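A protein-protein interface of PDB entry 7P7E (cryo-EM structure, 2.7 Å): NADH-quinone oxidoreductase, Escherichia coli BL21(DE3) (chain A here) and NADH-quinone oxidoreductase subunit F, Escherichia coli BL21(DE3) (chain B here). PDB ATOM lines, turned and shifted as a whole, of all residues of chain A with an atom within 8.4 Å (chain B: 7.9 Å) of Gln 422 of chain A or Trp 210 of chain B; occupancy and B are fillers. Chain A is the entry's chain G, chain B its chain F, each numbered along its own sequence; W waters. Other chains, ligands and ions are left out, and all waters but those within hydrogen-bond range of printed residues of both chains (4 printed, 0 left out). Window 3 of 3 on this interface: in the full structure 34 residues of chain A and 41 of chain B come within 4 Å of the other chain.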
ATOM      1  N   LYS A 399      27.312 -12.131  -3.888  1.00  0.00           N
ATOM      2  CA  LYS A 399      28.478 -11.422  -4.417  1.00  0.00           C
ATOM      3  C   LYS A 399      28.666 -10.065  -3.750  1.00  0.00           C
ATOM      4  O   LYS A 399      29.792  -9.696  -3.397  1.00  0.00           O
ATOM      5  CB  LYS A 399      28.375 -11.239  -5.930  1.00  0.00           C
ATOM      6  CG  LYS A 399      29.651 -10.645  -6.520  1.00  0.00           C
ATOM      7  CD  LYS A 399      29.560 -10.415  -8.010  1.00  0.00           C
ATOM      8  CE  LYS A 399      30.870  -9.886  -8.564  1.00  0.00           C
ATOM      9  NZ  LYS A 399      30.795  -9.657 -10.033  1.00  0.00           N
ATOM     10  N   ALA A 400      27.577  -9.304  -3.592  1.00  0.00           N
ATOM     11  CA  ALA A 400      27.642  -8.052  -2.847  1.00  0.00           C
ATOM     12  C   ALA A 400      28.072  -8.301  -1.412  1.00  0.00           C
ATOM     13  O   ALA A 400      28.842  -7.518  -0.839  1.00  0.00           O
ATOM     14  CB  ALA A 400      26.289  -7.346  -2.879  1.00  0.00           C
ATOM     15  N   MET A 403      31.989  -8.739  -1.650  1.00  0.00           N
ATOM     16  CA  MET A 403      32.734  -7.485  -1.788  1.00  0.00           C
ATOM     17  C   MET A 403      32.620  -6.612  -0.547  1.00  0.00           C
ATOM     18  O   MET A 403      33.550  -5.859  -0.241  1.00  0.00           O
ATOM     19  CB  MET A 403      32.296  -6.677  -3.015  1.00  0.00           C
ATOM     20  CG  MET A 403      31.814  -7.460  -4.205  1.00  0.00           C
ATOM     21  SD  MET A 403      30.937  -6.445  -5.410  1.00  0.00           S
ATOM     22  CE  MET A 403      31.848  -4.907  -5.310  1.00  0.00           C
ATOM     23  N   ALA A 415      22.673  -2.024   4.579  1.00  0.00           N
ATOM     24  CA  ALA A 415      22.691  -0.860   3.696  1.00  0.00           C
ATOM     25  C   ALA A 415      24.082  -0.614   3.123  1.00  0.00           C
ATOM     26  O   ALA A 415      24.222  -0.305   1.934  1.00  0.00           O
ATOM     27  CB  ALA A 415      22.190   0.374   4.443  1.00  0.00           C
ATOM     28  N   ALA A 416      25.121  -0.767   3.946  1.00  0.00           N
ATOM     29  CA  ALA A 416      26.491  -0.639   3.461  1.00  0.00           C
ATOM     30  C   ALA A 416      26.837  -1.737   2.461  1.00  0.00           C
ATOM     31  O   ALA A 416      27.524  -1.480   1.465  1.00  0.00           O
ATOM     32  CB  ALA A 416      27.463  -0.668   4.635  1.00  0.00           C
ATOM     33  N   ILE A 417      26.372  -2.963   2.718  1.00  0.00           N
ATOM     34  CA  ILE A 417      26.624  -4.080   1.811  1.00  0.00           C
ATOM     35  C   ILE A 417      25.974  -3.822   0.458  1.00  0.00           C
ATOM     36  O   ILE A 417      26.591  -4.019  -0.596  1.00  0.00           O
ATOM     37  CB  ILE A 417      26.118  -5.395   2.434  1.00  0.00           C
ATOM     38  CG1 ILE A 417      26.864  -5.698   3.733  1.00  0.00           C
ATOM     39  CG2 ILE A 417      26.250  -6.548   1.452  1.00  0.00           C
ATOM     40  CD1 ILE A 417      26.217  -6.761   4.572  1.00  0.00           C
ATOM     41  N   LEU A 418      24.723  -3.358   0.471  1.00  0.00           N
ATOM     42  CA  LEU A 418      24.020  -3.072  -0.775  1.00  0.00           C
ATOM     43  C   LEU A 418      24.614  -1.870  -1.497  1.00  0.00           C
ATOM     44  O   LEU A 418      24.582  -1.819  -2.731  1.00  0.00           O
ATOM     45  CB  LEU A 418      22.534  -2.844  -0.501  1.00  0.00           C
ATOM     46  CG  LEU A 418      21.732  -4.058  -0.025  1.00  0.00           C
ATOM     47  CD1 LEU A 418      20.258  -3.709   0.112  1.00  0.00           C
ATOM     48  CD2 LEU A 418      21.923  -5.235  -0.965  1.00  0.00           C
ATOM     49  N   ASN A 419      25.152  -0.899  -0.757  1.00  0.00           N
ATOM     50  CA  ASN A 419      25.792   0.239  -1.405  1.00  0.00           C
ATOM     51  C   ASN A 419      27.105  -0.164  -2.063  1.00  0.00           C
ATOM     52  O   ASN A 419      27.424   0.313  -3.158  1.00  0.00           O
ATOM     53  CB  ASN A 419      26.021   1.362  -0.397  1.00  0.00           C
ATOM     54  CG  ASN A 419      26.723   2.554  -1.009  1.00  0.00           C
ATOM     55  OD1 ASN A 419      26.219   3.170  -1.946  1.00  0.00           O
ATOM     56  ND2 ASN A 419      27.899   2.881  -0.489  1.00  0.00           N
ATOM     57  N   ILE A 420      27.883  -1.029  -1.410  1.00  0.00           N
ATOM     58  CA  ILE A 420      29.133  -1.500  -2.002  1.00  0.00           C
ATOM     59  C   ILE A 420      28.849  -2.368  -3.222  1.00  0.00           C
ATOM     60  O   ILE A 420      29.423  -2.166  -4.299  1.00  0.00           O
ATOM     61  CB  ILE A 420      29.972  -2.249  -0.952  1.00  0.00           C
ATOM     62  CG1 ILE A 420      30.570  -1.261   0.049  1.00  0.00           C
ATOM     63  CG2 ILE A 420      31.076  -3.058  -1.612  1.00  0.00           C
ATOM     64  CD1 ILE A 420      31.179  -1.914   1.261  1.00  0.00           C
ATOM     65  N   GLY A 421      27.952  -3.336  -3.076  1.00  0.00           N
ATOM     66  CA  GLY A 421      27.519  -4.165  -4.183  1.00  0.00           C
ATOM     67  C   GLY A 421      26.323  -3.585  -4.907  1.00  0.00           C
ATOM     68  O   GLY A 421      25.189  -4.008  -4.657  1.00  0.00           O
ATOM     69  N   GLN A 422      26.562  -2.592  -5.768  1.00  0.00           N
ATOM     70  CA  GLN A 422      25.476  -1.854  -6.410  1.00  0.00           C
ATOM     71  C   GLN A 422      24.612  -2.763  -7.277  1.00  0.00           C
ATOM     72  O   GLN A 422      23.443  -3.014  -6.966  1.00  0.00           O
ATOM     73  CB  GLN A 422      26.057  -0.714  -7.244  1.00  0.00           C
ATOM     74  CG  GLN A 422      26.624   0.415  -6.424  1.00  0.00           C
ATOM     75  CD  GLN A 422      25.560   1.390  -5.983  1.00  0.00           C
ATOM     76  OE1 GLN A 422      24.783   1.885  -6.797  1.00  0.00           O
ATOM     77  NE2 GLN A 422      25.515   1.672  -4.690  1.00  0.00           N
ATOM     78  N   ARG A 423      25.177  -3.276  -8.367  1.00  0.00           N
ATOM     79  CA  ARG A 423      24.476  -4.223  -9.221  1.00  0.00           C
ATOM     80  C   ARG A 423      25.322  -5.453  -9.515  1.00  0.00           C
ATOM     81  O   ARG A 423      24.908  -6.299 -10.314  1.00  0.00           O
ATOM     82  CB  ARG A 423      24.039  -3.561 -10.535  1.00  0.00           C
ATOM     83  CG  ARG A 423      22.871  -2.604 -10.389  1.00  0.00           C
ATOM     84  CD  ARG A 423      22.675  -1.771 -11.643  1.00  0.00           C
ATOM     85  NE  ARG A 423      23.744  -0.797 -11.825  1.00  0.00           N
ATOM     86  CZ  ARG A 423      23.909  -0.061 -12.917  1.00  0.00           C
ATOM     87  NH1 ARG A 423      23.088  -0.162 -13.949  1.00  0.00           N
ATOM     88  NH2 ARG A 423      24.924   0.796 -12.974  1.00  0.00           N
ATOM     89  N   ALA A 424      26.495  -5.568  -8.898  1.00  0.00           N
ATOM     90  CA  ALA A 424      27.315  -6.758  -9.055  1.00  0.00           C
ATOM     91  C   ALA A 424      26.653  -7.930  -8.349  1.00  0.00           C
ATOM     92  O   ALA A 424      26.258  -7.826  -7.185  1.00  0.00           O
ATOM     93  CB  ALA A 424      28.713  -6.518  -8.493  1.00  0.00           C
ATOM     94  N   LYS A 425      26.532  -9.050  -9.054  1.00  0.00           N
ATOM     95  CA  LYS A 425      25.810 -10.190  -8.519  1.00  0.00           C
ATOM     96  C   LYS A 425      26.421 -11.474  -9.054  1.00  0.00           C
ATOM     97  O   LYS A 425      27.112 -11.482 -10.076  1.00  0.00           O
ATOM     98  CB  LYS A 425      24.320 -10.115  -8.862  1.00  0.00           C
ATOM     99  CG  LYS A 425      24.018 -10.059 -10.343  1.00  0.00           C
ATOM    100  CD  LYS A 425      22.526  -9.932 -10.589  1.00  0.00           C
ATOM    101  CE  LYS A 425      21.995  -8.611 -10.070  1.00  0.00           C
ATOM    102  NZ  LYS A 425      20.602  -8.357 -10.517  1.00  0.00           N
ATOM    103  N   ILE B  84      37.594   4.874  -9.440  1.00  0.00           N
ATOM    104  CA  ILE B  84      36.359   5.471  -9.938  1.00  0.00           C
ATOM    105  C   ILE B  84      35.889   6.487  -8.903  1.00  0.00           C
ATOM    106  O   ILE B  84      34.689   6.628  -8.646  1.00  0.00           O
ATOM    107  CB  ILE B  84      35.284   4.403 -10.229  1.00  0.00           C
ATOM    108  CG1 ILE B  84      35.926   3.107 -10.731  1.00  0.00           C
ATOM    109  CG2 ILE B  84      34.293   4.896 -11.280  1.00  0.00           C
ATOM    110  CD1 ILE B  84      36.478   3.190 -12.144  1.00  0.00           C
ATOM    111  N   TYR B  86      34.988   9.920  -6.810  1.00  0.00           N
ATOM    112  CA  TYR B  86      34.069  11.000  -7.143  1.00  0.00           C
ATOM    113  C   TYR B  86      34.271  12.190  -6.219  1.00  0.00           C
ATOM    114  O   TYR B  86      34.550  12.029  -5.023  1.00  0.00           O
ATOM    115  CB  TYR B  86      32.613  10.540  -7.046  1.00  0.00           C
ATOM    116  CG  TYR B  86      32.183   9.614  -8.152  1.00  0.00           C
ATOM    117  CD1 TYR B  86      31.936  10.094  -9.428  1.00  0.00           C
ATOM    118  CD2 TYR B  86      32.017   8.257  -7.918  1.00  0.00           C
ATOM    119  CE1 TYR B  86      31.539   9.250 -10.442  1.00  0.00           C
ATOM    120  CE2 TYR B  86      31.620   7.404  -8.925  1.00  0.00           C
ATOM    121  CZ  TYR B  86      31.384   7.906 -10.184  1.00  0.00           C
ATOM    122  OH  TYR B  86      30.989   7.059 -11.190  1.00  0.00           O
ATOM    123  N   LEU B  88      32.151  15.619  -4.993  1.00  0.00           N
ATOM    124  CA  LEU B  88      30.828  16.225  -4.958  1.00  0.00           C
ATOM    125  C   LEU B  88      30.909  17.567  -4.246  1.00  0.00           C
ATOM    126  O   LEU B  88      31.553  17.683  -3.198  1.00  0.00           O
ATOM    127  CB  LEU B  88      29.817  15.308  -4.261  1.00  0.00           C
ATOM    128  CG  LEU B  88      29.783  13.838  -4.691  1.00  0.00           C
ATOM    129  CD1 LEU B  88      28.646  13.108  -4.007  1.00  0.00           C
ATOM    130  CD2 LEU B  88      29.660  13.701  -6.195  1.00  0.00           C
ATOM    131  N   TYR B 126      37.864  11.208 -11.192  1.00  0.00           N
ATOM    132  CA  TYR B 126      37.641  11.477 -12.605  1.00  0.00           C
ATOM    133  C   TYR B 126      36.356  12.245 -12.871  1.00  0.00           C
ATOM    134  O   TYR B 126      36.177  12.749 -13.984  1.00  0.00           O
ATOM    135  CB  TYR B 126      37.627  10.163 -13.393  1.00  0.00           C
ATOM    136  CG  TYR B 126      36.293   9.447 -13.399  1.00  0.00           C
ATOM    137  CD1 TYR B 126      35.706   9.012 -12.215  1.00  0.00           C
ATOM    138  CD2 TYR B 126      35.626   9.198 -14.589  1.00  0.00           C
ATOM    139  CE1 TYR B 126      34.492   8.362 -12.220  1.00  0.00           C
ATOM    140  CE2 TYR B 126      34.412   8.543 -14.603  1.00  0.00           C
ATOM    141  CZ  TYR B 126      33.851   8.128 -13.416  1.00  0.00           C
ATOM    142  OH  TYR B 126      32.640   7.476 -13.422  1.00  0.00           O
ATOM    143  N   ARG B 127      35.460  12.347 -11.892  1.00  0.00           N
ATOM    144  CA  ARG B 127      34.176  12.994 -12.105  1.00  0.00           C
ATOM    145  C   ARG B 127      33.823  13.881 -10.923  1.00  0.00           C
ATOM    146  O   ARG B 127      34.067  13.528  -9.762  1.00  0.00           O
ATOM    147  CB  ARG B 127      33.066  11.966 -12.331  1.00  0.00           C
ATOM    148  CG  ARG B 127      32.790  11.703 -13.792  1.00  0.00           C
ATOM    149  CD  ARG B 127      31.575  10.832 -13.998  1.00  0.00           C
ATOM    150  NE  ARG B 127      31.334  10.594 -15.415  1.00  0.00           N
ATOM    151  CZ  ARG B 127      30.500   9.683 -15.891  1.00  0.00           C
ATOM    152  NH1 ARG B 127      29.805   8.895 -15.088  1.00  0.00           N
ATOM    153  NH2 ARG B 127      30.361   9.556 -17.208  1.00  0.00           N
ATOM    154  N   TYR B 129      30.537  16.379  -9.409  1.00  0.00           N
ATOM    155  CA  TYR B 129      29.124  16.728  -9.485  1.00  0.00           C
ATOM    156  C   TYR B 129      28.858  17.888  -8.542  1.00  0.00           C
ATOM    157  O   TYR B 129      29.163  17.800  -7.351  1.00  0.00           O
ATOM    158  CB  TYR B 129      28.238  15.536  -9.119  1.00  0.00           C
ATOM    159  CG  TYR B 129      28.264  14.406 -10.118  1.00  0.00           C
ATOM    160  CD1 TYR B 129      27.435  14.419 -11.231  1.00  0.00           C
ATOM    161  CD2 TYR B 129      29.109  13.321  -9.943  1.00  0.00           C
ATOM    162  CE1 TYR B 129      27.453  13.387 -12.143  1.00  0.00           C
ATOM    163  CE2 TYR B 129      29.134  12.284 -10.850  1.00  0.00           C
ATOM    164  CZ  TYR B 129      28.304  12.322 -11.947  1.00  0.00           C
ATOM    165  OH  TYR B 129      28.323  11.292 -12.854  1.00  0.00           O
ATOM    166  N   HIS B 172      24.133  19.010 -11.098  1.00  0.00           N
ATOM    167  CA  HIS B 172      22.916  18.276 -10.783  1.00  0.00           C
ATOM    168  C   HIS B 172      22.008  19.203  -9.985  1.00  0.00           C
ATOM    169  O   HIS B 172      22.291  19.504  -8.821  1.00  0.00           O
ATOM    170  CB  HIS B 172      23.250  17.004 -10.003  1.00  0.00           C
ATOM    171  CG  HIS B 172      22.053  16.257  -9.502  1.00  0.00           C
ATOM    172  ND1 HIS B 172      21.526  15.170 -10.164  1.00  0.00           N
ATOM    173  CD2 HIS B 172      21.295  16.423  -8.392  1.00  0.00           C
ATOM    174  CE1 HIS B 172      20.487  14.708  -9.491  1.00  0.00           C
ATOM    175  NE2 HIS B 172      20.325  15.453  -8.413  1.00  0.00           N
ATOM    176  N   ILE B 187      24.546  12.073  -1.262  1.00  0.00           N
ATOM    177  CA  ILE B 187      24.980  10.951  -2.089  1.00  0.00           C
ATOM    178  C   ILE B 187      23.783  10.119  -2.528  1.00  0.00           C
ATOM    179  O   ILE B 187      23.693   9.694  -3.687  1.00  0.00           O
ATOM    180  CB  ILE B 187      26.017  10.111  -1.321  1.00  0.00           C
ATOM    181  CG1 ILE B 187      27.324  10.887  -1.189  1.00  0.00           C
ATOM    182  CG2 ILE B 187      26.268   8.792  -2.006  1.00  0.00           C
ATOM    183  CD1 ILE B 187      28.195  10.392  -0.082  1.00  0.00           C
ATOM    184  N   ASN B 188      22.837   9.889  -1.612  1.00  0.00           N
ATOM    185  CA  ASN B 188      21.630   9.139  -1.950  1.00  0.00           C
ATOM    186  C   ASN B 188      20.788   9.863  -2.997  1.00  0.00           C
ATOM    187  O   ASN B 188      20.253   9.231  -3.913  1.00  0.00           O
ATOM    188  CB  ASN B 188      20.805   8.875  -0.693  1.00  0.00           C
ATOM    189  CG  ASN B 188      20.968   7.462  -0.177  1.00  0.00           C
ATOM    190  OD1 ASN B 188      21.297   6.549  -0.931  1.00  0.00           O
ATOM    191  ND2 ASN B 188      20.736   7.273   1.114  1.00  0.00           N
ATOM    192  N   SER B 189      20.658  11.187  -2.880  1.00  0.00           N
ATOM    193  CA  SER B 189      19.872  11.934  -3.858  1.00  0.00           C
ATOM    194  C   SER B 189      20.589  12.044  -5.197  1.00  0.00           C
ATOM    195  O   SER B 189      19.934  12.150  -6.239  1.00  0.00           O
ATOM    196  CB  SER B 189      19.536  13.325  -3.327  1.00  0.00           C
ATOM    197  OG  SER B 189      20.606  13.859  -2.577  1.00  0.00           O
ATOM    198  N   LEU B 190      21.924  12.033  -5.189  1.00  0.00           N
ATOM    199  CA  LEU B 190      22.675  12.020  -6.439  1.00  0.00           C
ATOM    200  C   LEU B 190      22.465  10.718  -7.199  1.00  0.00           C
ATOM    201  O   LEU B 190      22.441  10.720  -8.434  1.00  0.00           O
ATOM    202  CB  LEU B 190      24.159  12.245  -6.161  1.00  0.00           C
ATOM    203  CG  LEU B 190      25.087  12.294  -7.375  1.00  0.00           C
ATOM    204  CD1 LEU B 190      25.026  13.653  -8.047  1.00  0.00           C
ATOM    205  CD2 LEU B 190      26.503  11.946  -6.973  1.00  0.00           C
ATOM    206  N   GLU B 191      22.282   9.611  -6.486  1.00  0.00           N
ATOM    207  CA  GLU B 191      22.010   8.314  -7.090  1.00  0.00           C
ATOM    208  C   GLU B 191      20.559   8.152  -7.528  1.00  0.00           C
ATOM    209  O   GLU B 191      20.181   7.062  -7.968  1.00  0.00           O
ATOM    210  CB  GLU B 191      22.382   7.193  -6.116  1.00  0.00           C
ATOM    211  CG  GLU B 191      23.862   7.112  -5.796  1.00  0.00           C
ATOM    212  CD  GLU B 191      24.183   6.007  -4.811  1.00  0.00           C
ATOM    213  OE1 GLU B 191      23.275   5.221  -4.479  1.00  0.00           O
ATOM    214  OE2 GLU B 191      25.345   5.926  -4.367  1.00  0.00           O
ATOM    215  N   GLY B 192      19.743   9.198  -7.424  1.00  0.00           N
ATOM    216  CA  GLY B 192      18.361   9.117  -7.844  1.00  0.00           C
ATOM    217  C   GLY B 192      17.438   8.427  -6.873  1.00  0.00           C
ATOM    218  O   GLY B 192      16.402   7.904  -7.288  1.00  0.00           O
ATOM    219  N   ARG B 193      17.780   8.404  -5.593  1.00  0.00           N
ATOM    220  CA  ARG B 193      16.982   7.752  -4.568  1.00  0.00           C
ATOM    221  C   ARG B 193      16.357   8.800  -3.655  1.00  0.00           C
ATOM    222  O   ARG B 193      16.614  10.001  -3.777  1.00  0.00           O
ATOM    223  CB  ARG B 193      17.837   6.772  -3.764  1.00  0.00           C
ATOM    224  CG  ARG B 193      18.655   5.821  -4.606  1.00  0.00           C
ATOM    225  CD  ARG B 193      19.554   4.963  -3.733  1.00  0.00           C
ATOM    226  NE  ARG B 193      20.276   3.961  -4.505  1.00  0.00           N
ATOM    227  CZ  ARG B 193      19.759   2.811  -4.915  1.00  0.00           C
ATOM    228  NH1 ARG B 193      18.509   2.478  -4.641  1.00  0.00           N
ATOM    229  NH2 ARG B 193      20.514   1.975  -5.619  1.00  0.00           N
ATOM    230  N   ARG B 198      22.847   8.020   5.406  1.00  0.00           N
ATOM    231  CA  ARG B 198      23.425   6.703   5.611  1.00  0.00           C
ATOM    232  C   ARG B 198      24.139   6.646   6.953  1.00  0.00           C
ATOM    233  O   ARG B 198      24.576   7.669   7.487  1.00  0.00           O
ATOM    234  CB  ARG B 198      24.409   6.351   4.496  1.00  0.00           C
ATOM    235  CG  ARG B 198      23.838   6.485   3.107  1.00  0.00           C
ATOM    236  CD  ARG B 198      24.917   6.299   2.068  1.00  0.00           C
ATOM    237  NE  ARG B 198      24.360   6.168   0.730  1.00  0.00           N
ATOM    238  CZ  ARG B 198      25.078   5.935  -0.357  1.00  0.00           C
ATOM    239  NH1 ARG B 198      26.391   5.797  -0.300  1.00  0.00           N
ATOM    240  NH2 ARG B 198      24.464   5.842  -1.532  1.00  0.00           N
ATOM    241  N   SER B 207      33.390   4.069   0.628  1.00  0.00           N
ATOM    242  CA  SER B 207      32.286   3.614  -0.216  1.00  0.00           C
ATOM    243  C   SER B 207      31.192   4.678  -0.162  1.00  0.00           C
ATOM    244  O   SER B 207      30.372   4.682   0.760  1.00  0.00           O
ATOM    245  CB  SER B 207      31.769   2.255   0.233  1.00  0.00           C
ATOM    246  OG  SER B 207      31.373   2.279   1.592  1.00  0.00           O
ATOM    247  N   GLY B 208      31.190   5.569  -1.148  1.00  0.00           N
ATOM    248  CA  GLY B 208      30.242   6.663  -1.181  1.00  0.00           C
ATOM    249  C   GLY B 208      29.277   6.594  -2.343  1.00  0.00           C
ATOM    250  O   GLY B 208      28.340   5.792  -2.332  1.00  0.00           O
ATOM    251  N   ALA B 209      29.495   7.438  -3.349  1.00  0.00           N
ATOM    252  CA  ALA B 209      28.611   7.492  -4.505  1.00  0.00           C
ATOM    253  C   ALA B 209      28.795   6.248  -5.361  1.00  0.00           C
ATOM    254  O   ALA B 209      29.893   5.995  -5.869  1.00  0.00           O
ATOM    255  CB  ALA B 209      28.880   8.754  -5.319  1.00  0.00           C
ATOM    256  N   TRP B 210      27.714   5.473  -5.505  1.00  0.00           N
ATOM    257  CA  TRP B 210      27.687   4.213  -6.252  1.00  0.00           C
ATOM    258  C   TRP B 210      28.720   3.215  -5.734  1.00  0.00           C
ATOM    259  O   TRP B 210      29.275   2.426  -6.500  1.00  0.00           O
ATOM    260  CB  TRP B 210      27.868   4.449  -7.756  1.00  0.00           C
ATOM    261  CG  TRP B 210      26.817   5.340  -8.342  1.00  0.00           C
ATOM    262  CD1 TRP B 210      25.534   5.001  -8.641  1.00  0.00           C
ATOM    263  CD2 TRP B 210      26.959   6.721  -8.693  1.00  0.00           C
ATOM    264  NE1 TRP B 210      24.867   6.082  -9.158  1.00  0.00           N
ATOM    265  CE2 TRP B 210      25.720   7.151  -9.201  1.00  0.00           C
ATOM    266  CE3 TRP B 210      28.015   7.634  -8.629  1.00  0.00           C
ATOM    267  CZ2 TRP B 210      25.506   8.453  -9.640  1.00  0.00           C
ATOM    268  CZ3 TRP B 210      27.800   8.926  -9.066  1.00  0.00           C
ATOM    269  CH2 TRP B 210      26.557   9.324  -9.565  1.00  0.00           C
ATOM    270  N   GLY B 211      28.986   3.245  -4.431  1.00  0.00           N
ATOM    271  CA  GLY B 211      29.932   2.343  -3.814  1.00  0.00           C
ATOM    272  C   GLY B 211      31.388   2.704  -3.994  1.00  0.00           C
ATOM    273  O   GLY B 211      32.252   1.968  -3.505  1.00  0.00           O
ATOM    274  N   LYS B 212      31.688   3.799  -4.670  1.00  0.00           N
ATOM    275  CA  LYS B 212      33.051   4.217  -4.944  1.00  0.00           C
ATOM    276  C   LYS B 212      33.530   5.199  -3.887  1.00  0.00           C
ATOM    277  O   LYS B 212      32.722   5.768  -3.148  1.00  0.00           O
ATOM    278  CB  LYS B 212      33.130   4.856  -6.328  1.00  0.00           C
ATOM    279  CG  LYS B 212      32.548   4.001  -7.434  1.00  0.00           C
ATOM    280  CD  LYS B 212      33.251   2.662  -7.524  1.00  0.00           C
ATOM    281  CE  LYS B 212      32.728   1.846  -8.689  1.00  0.00           C
ATOM    282  NZ  LYS B 212      31.292   1.496  -8.516  1.00  0.00           N
ATOM    283  N   PRO B 213      34.845   5.371  -3.747  1.00  0.00           N
ATOM    284  CA  PRO B 213      35.364   6.456  -2.903  1.00  0.00           C
ATOM    285  C   PRO B 213      34.851   7.811  -3.368  1.00  0.00           C
ATOM    286  O   PRO B 213      34.848   8.120  -4.560  1.00  0.00           O
ATOM    287  CB  PRO B 213      36.885   6.338  -3.062  1.00  0.00           C
ATOM    288  CG  PRO B 213      37.132   5.142  -3.935  1.00  0.00           C
ATOM    289  CD  PRO B 213      35.878   4.366  -4.033  1.00  0.00           C
ATOM    290  N   THR B 214      34.409   8.620  -2.411  1.00  0.00           N
ATOM    291  CA  THR B 214      33.668   9.835  -2.713  1.00  0.00           C
ATOM    292  C   THR B 214      33.971  10.868  -1.642  1.00  0.00           C
ATOM    293  O   THR B 214      33.963  10.542  -0.452  1.00  0.00           O
ATOM    294  CB  THR B 214      32.160   9.548  -2.774  1.00  0.00           C
ATOM    295  OG1 THR B 214      31.885   8.646  -3.852  1.00  0.00           O
ATOM    296  CG2 THR B 214      31.364  10.818  -2.984  1.00  0.00           C
HETATM  297  O   HOH W   1      32.143  -0.823  -4.671  1.00  0.00           O
HETATM  298  O   HOH W   2      23.560   2.733  -2.615  1.00  0.00           O
HETATM  299  O   HOH W   3      22.815   3.386  -7.029  1.00  0.00           O
HETATM  300  O   HOH W   4      28.637   1.248   1.658  1.00  0.00           O
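O of Ser 207 of chain B sits at hydrogen-bond distance from ND2 of Asn 419 of chain A (3.3 Å).
The backbone carbonyl oxygen (O) of Gly 208 of chain B lies close to the side-chain amide oxygen (OD1) of Asn 419 of chain A, 3.4 Å away.
The side-chain amide oxygen (OD1) of Asn 419 of chain A lies within hydrogen-bond range of the guanidinium group (NH1) of Arg 198 of chain B.
The backbone carbonyl oxygen of Trp 210 of chain B is in hydrogen-bond range of the side-chain amino group of Lys 212 of chain B.
OD1 of Asn 188 of chain B sits at hydrogen-bond distance from NH2 of Arg 198 of chain B (3.3 Å).
NE of Arg 193 of chain B lies within salt-bridge range of OE1 of Glu 191 of chain B, at 3.3 Å.
The side-chain carboxylate of Glu 191 of chain B sits at hydrogen-bond distance from the backbone NH of Trp 210 of chain B (2.7 Å).
O of Asn 419 of chain A lies within hydrogen-bond range of NE2 of Gln 422 of chain A.
OE2 of Glu 191 of chain B is in salt-bridge range of NH2 of Arg 198 of chain B.
Glu 191 of chain B touches Asn 419 of chain A.
Gly 211 of chain B touches Asn 419 of chain A.
Ile 420 of chain A touches Ser 207 of chain B.
Trp 210 of chain B touches Gln 422 of chain A.
Gln 422 of chain A touches Gly 211 of chain B (NE2 to N, 3.8 Å).
Of the printed residues of chain B, Ile 420 of chain A touches Ser 207 (3.7 Å).
No residue of chain B comes within 4 Å of Gly 421 of chain A.
Of the printed residues of chain B, Gln 422 of chain A touches Trp 210 and Gly 211.
His 172 of chain B touches none of the printed residues of chain A.
Ile 187 of chain B touches none of the printed residues of chain A.
Of the printed residues of chain A, Glu 191 of chain B touches Asn 419 (3.8 Å).
Of the printed residues of chain A, Arg 198 of chain B touches Asn 419 (3.1 Å).
Of the printed residues of chain A, Gly 208 of chain B touches Asn 419 (3.4 Å).
No residue of chain A comes within 4 Å of Ala 209 of chain B.
Of chain A, only Gln 422 comes within 4 Å of Trp 210 of chain B.
The nearest residue of chain B that does not touch Gln 422 of chain A is Glu 191 of chain B (4.2 Å).
The nearest residue of chain A that does not touch Trp 210 of chain B is Asn 419 of chain A (4.1 Å).
The nearest printed residue of chain A that does not touch Arg 198 of chain B is Gln 422 of chain A (5.3 Å).
Of the 23 printed residues of chain B, 6 touch a printed residue of chain A.
Hydrophobic or aromatic side chains of chain A within 4 Å of the printed part of chain B: Ile 420.
Among the printed residues, 8 pairs touch across the chains.
Among the printed residues, no Asp or Glu carboxylate lies within 4 Å of a Lys or Arg side-chain nitrogen of the other chain.
Water W3 lies within hydrogen-bond range of OE1 of Gln 422 of chain A (2.5 Å), NH2 of Arg 193 of chain B (3.0 Å) and OE1 of Glu 191 of chain B (3.2 Å).
Water W2 lies within hydrogen-bond range of the side-chain amide oxygen of Asn 419 of chain A, the side-chain amide nitrogen of Gln 422 of chain A, the side-chain carboxylate of Glu 191 of chain B and the guanidinium group of Arg 198 of chain B.
Water W4 lies within hydrogen-bond range of the side-chain amide nitrogen of Asn 419 of chain A, the side-chain hydroxyl of Ser 207 of chain B and the backbone carbonyl oxygen of Ala 416 of chain A.
Water W1 lies within hydrogen-bond range of O of Gly 211 of chain B and O of Ile 420 of chain A.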
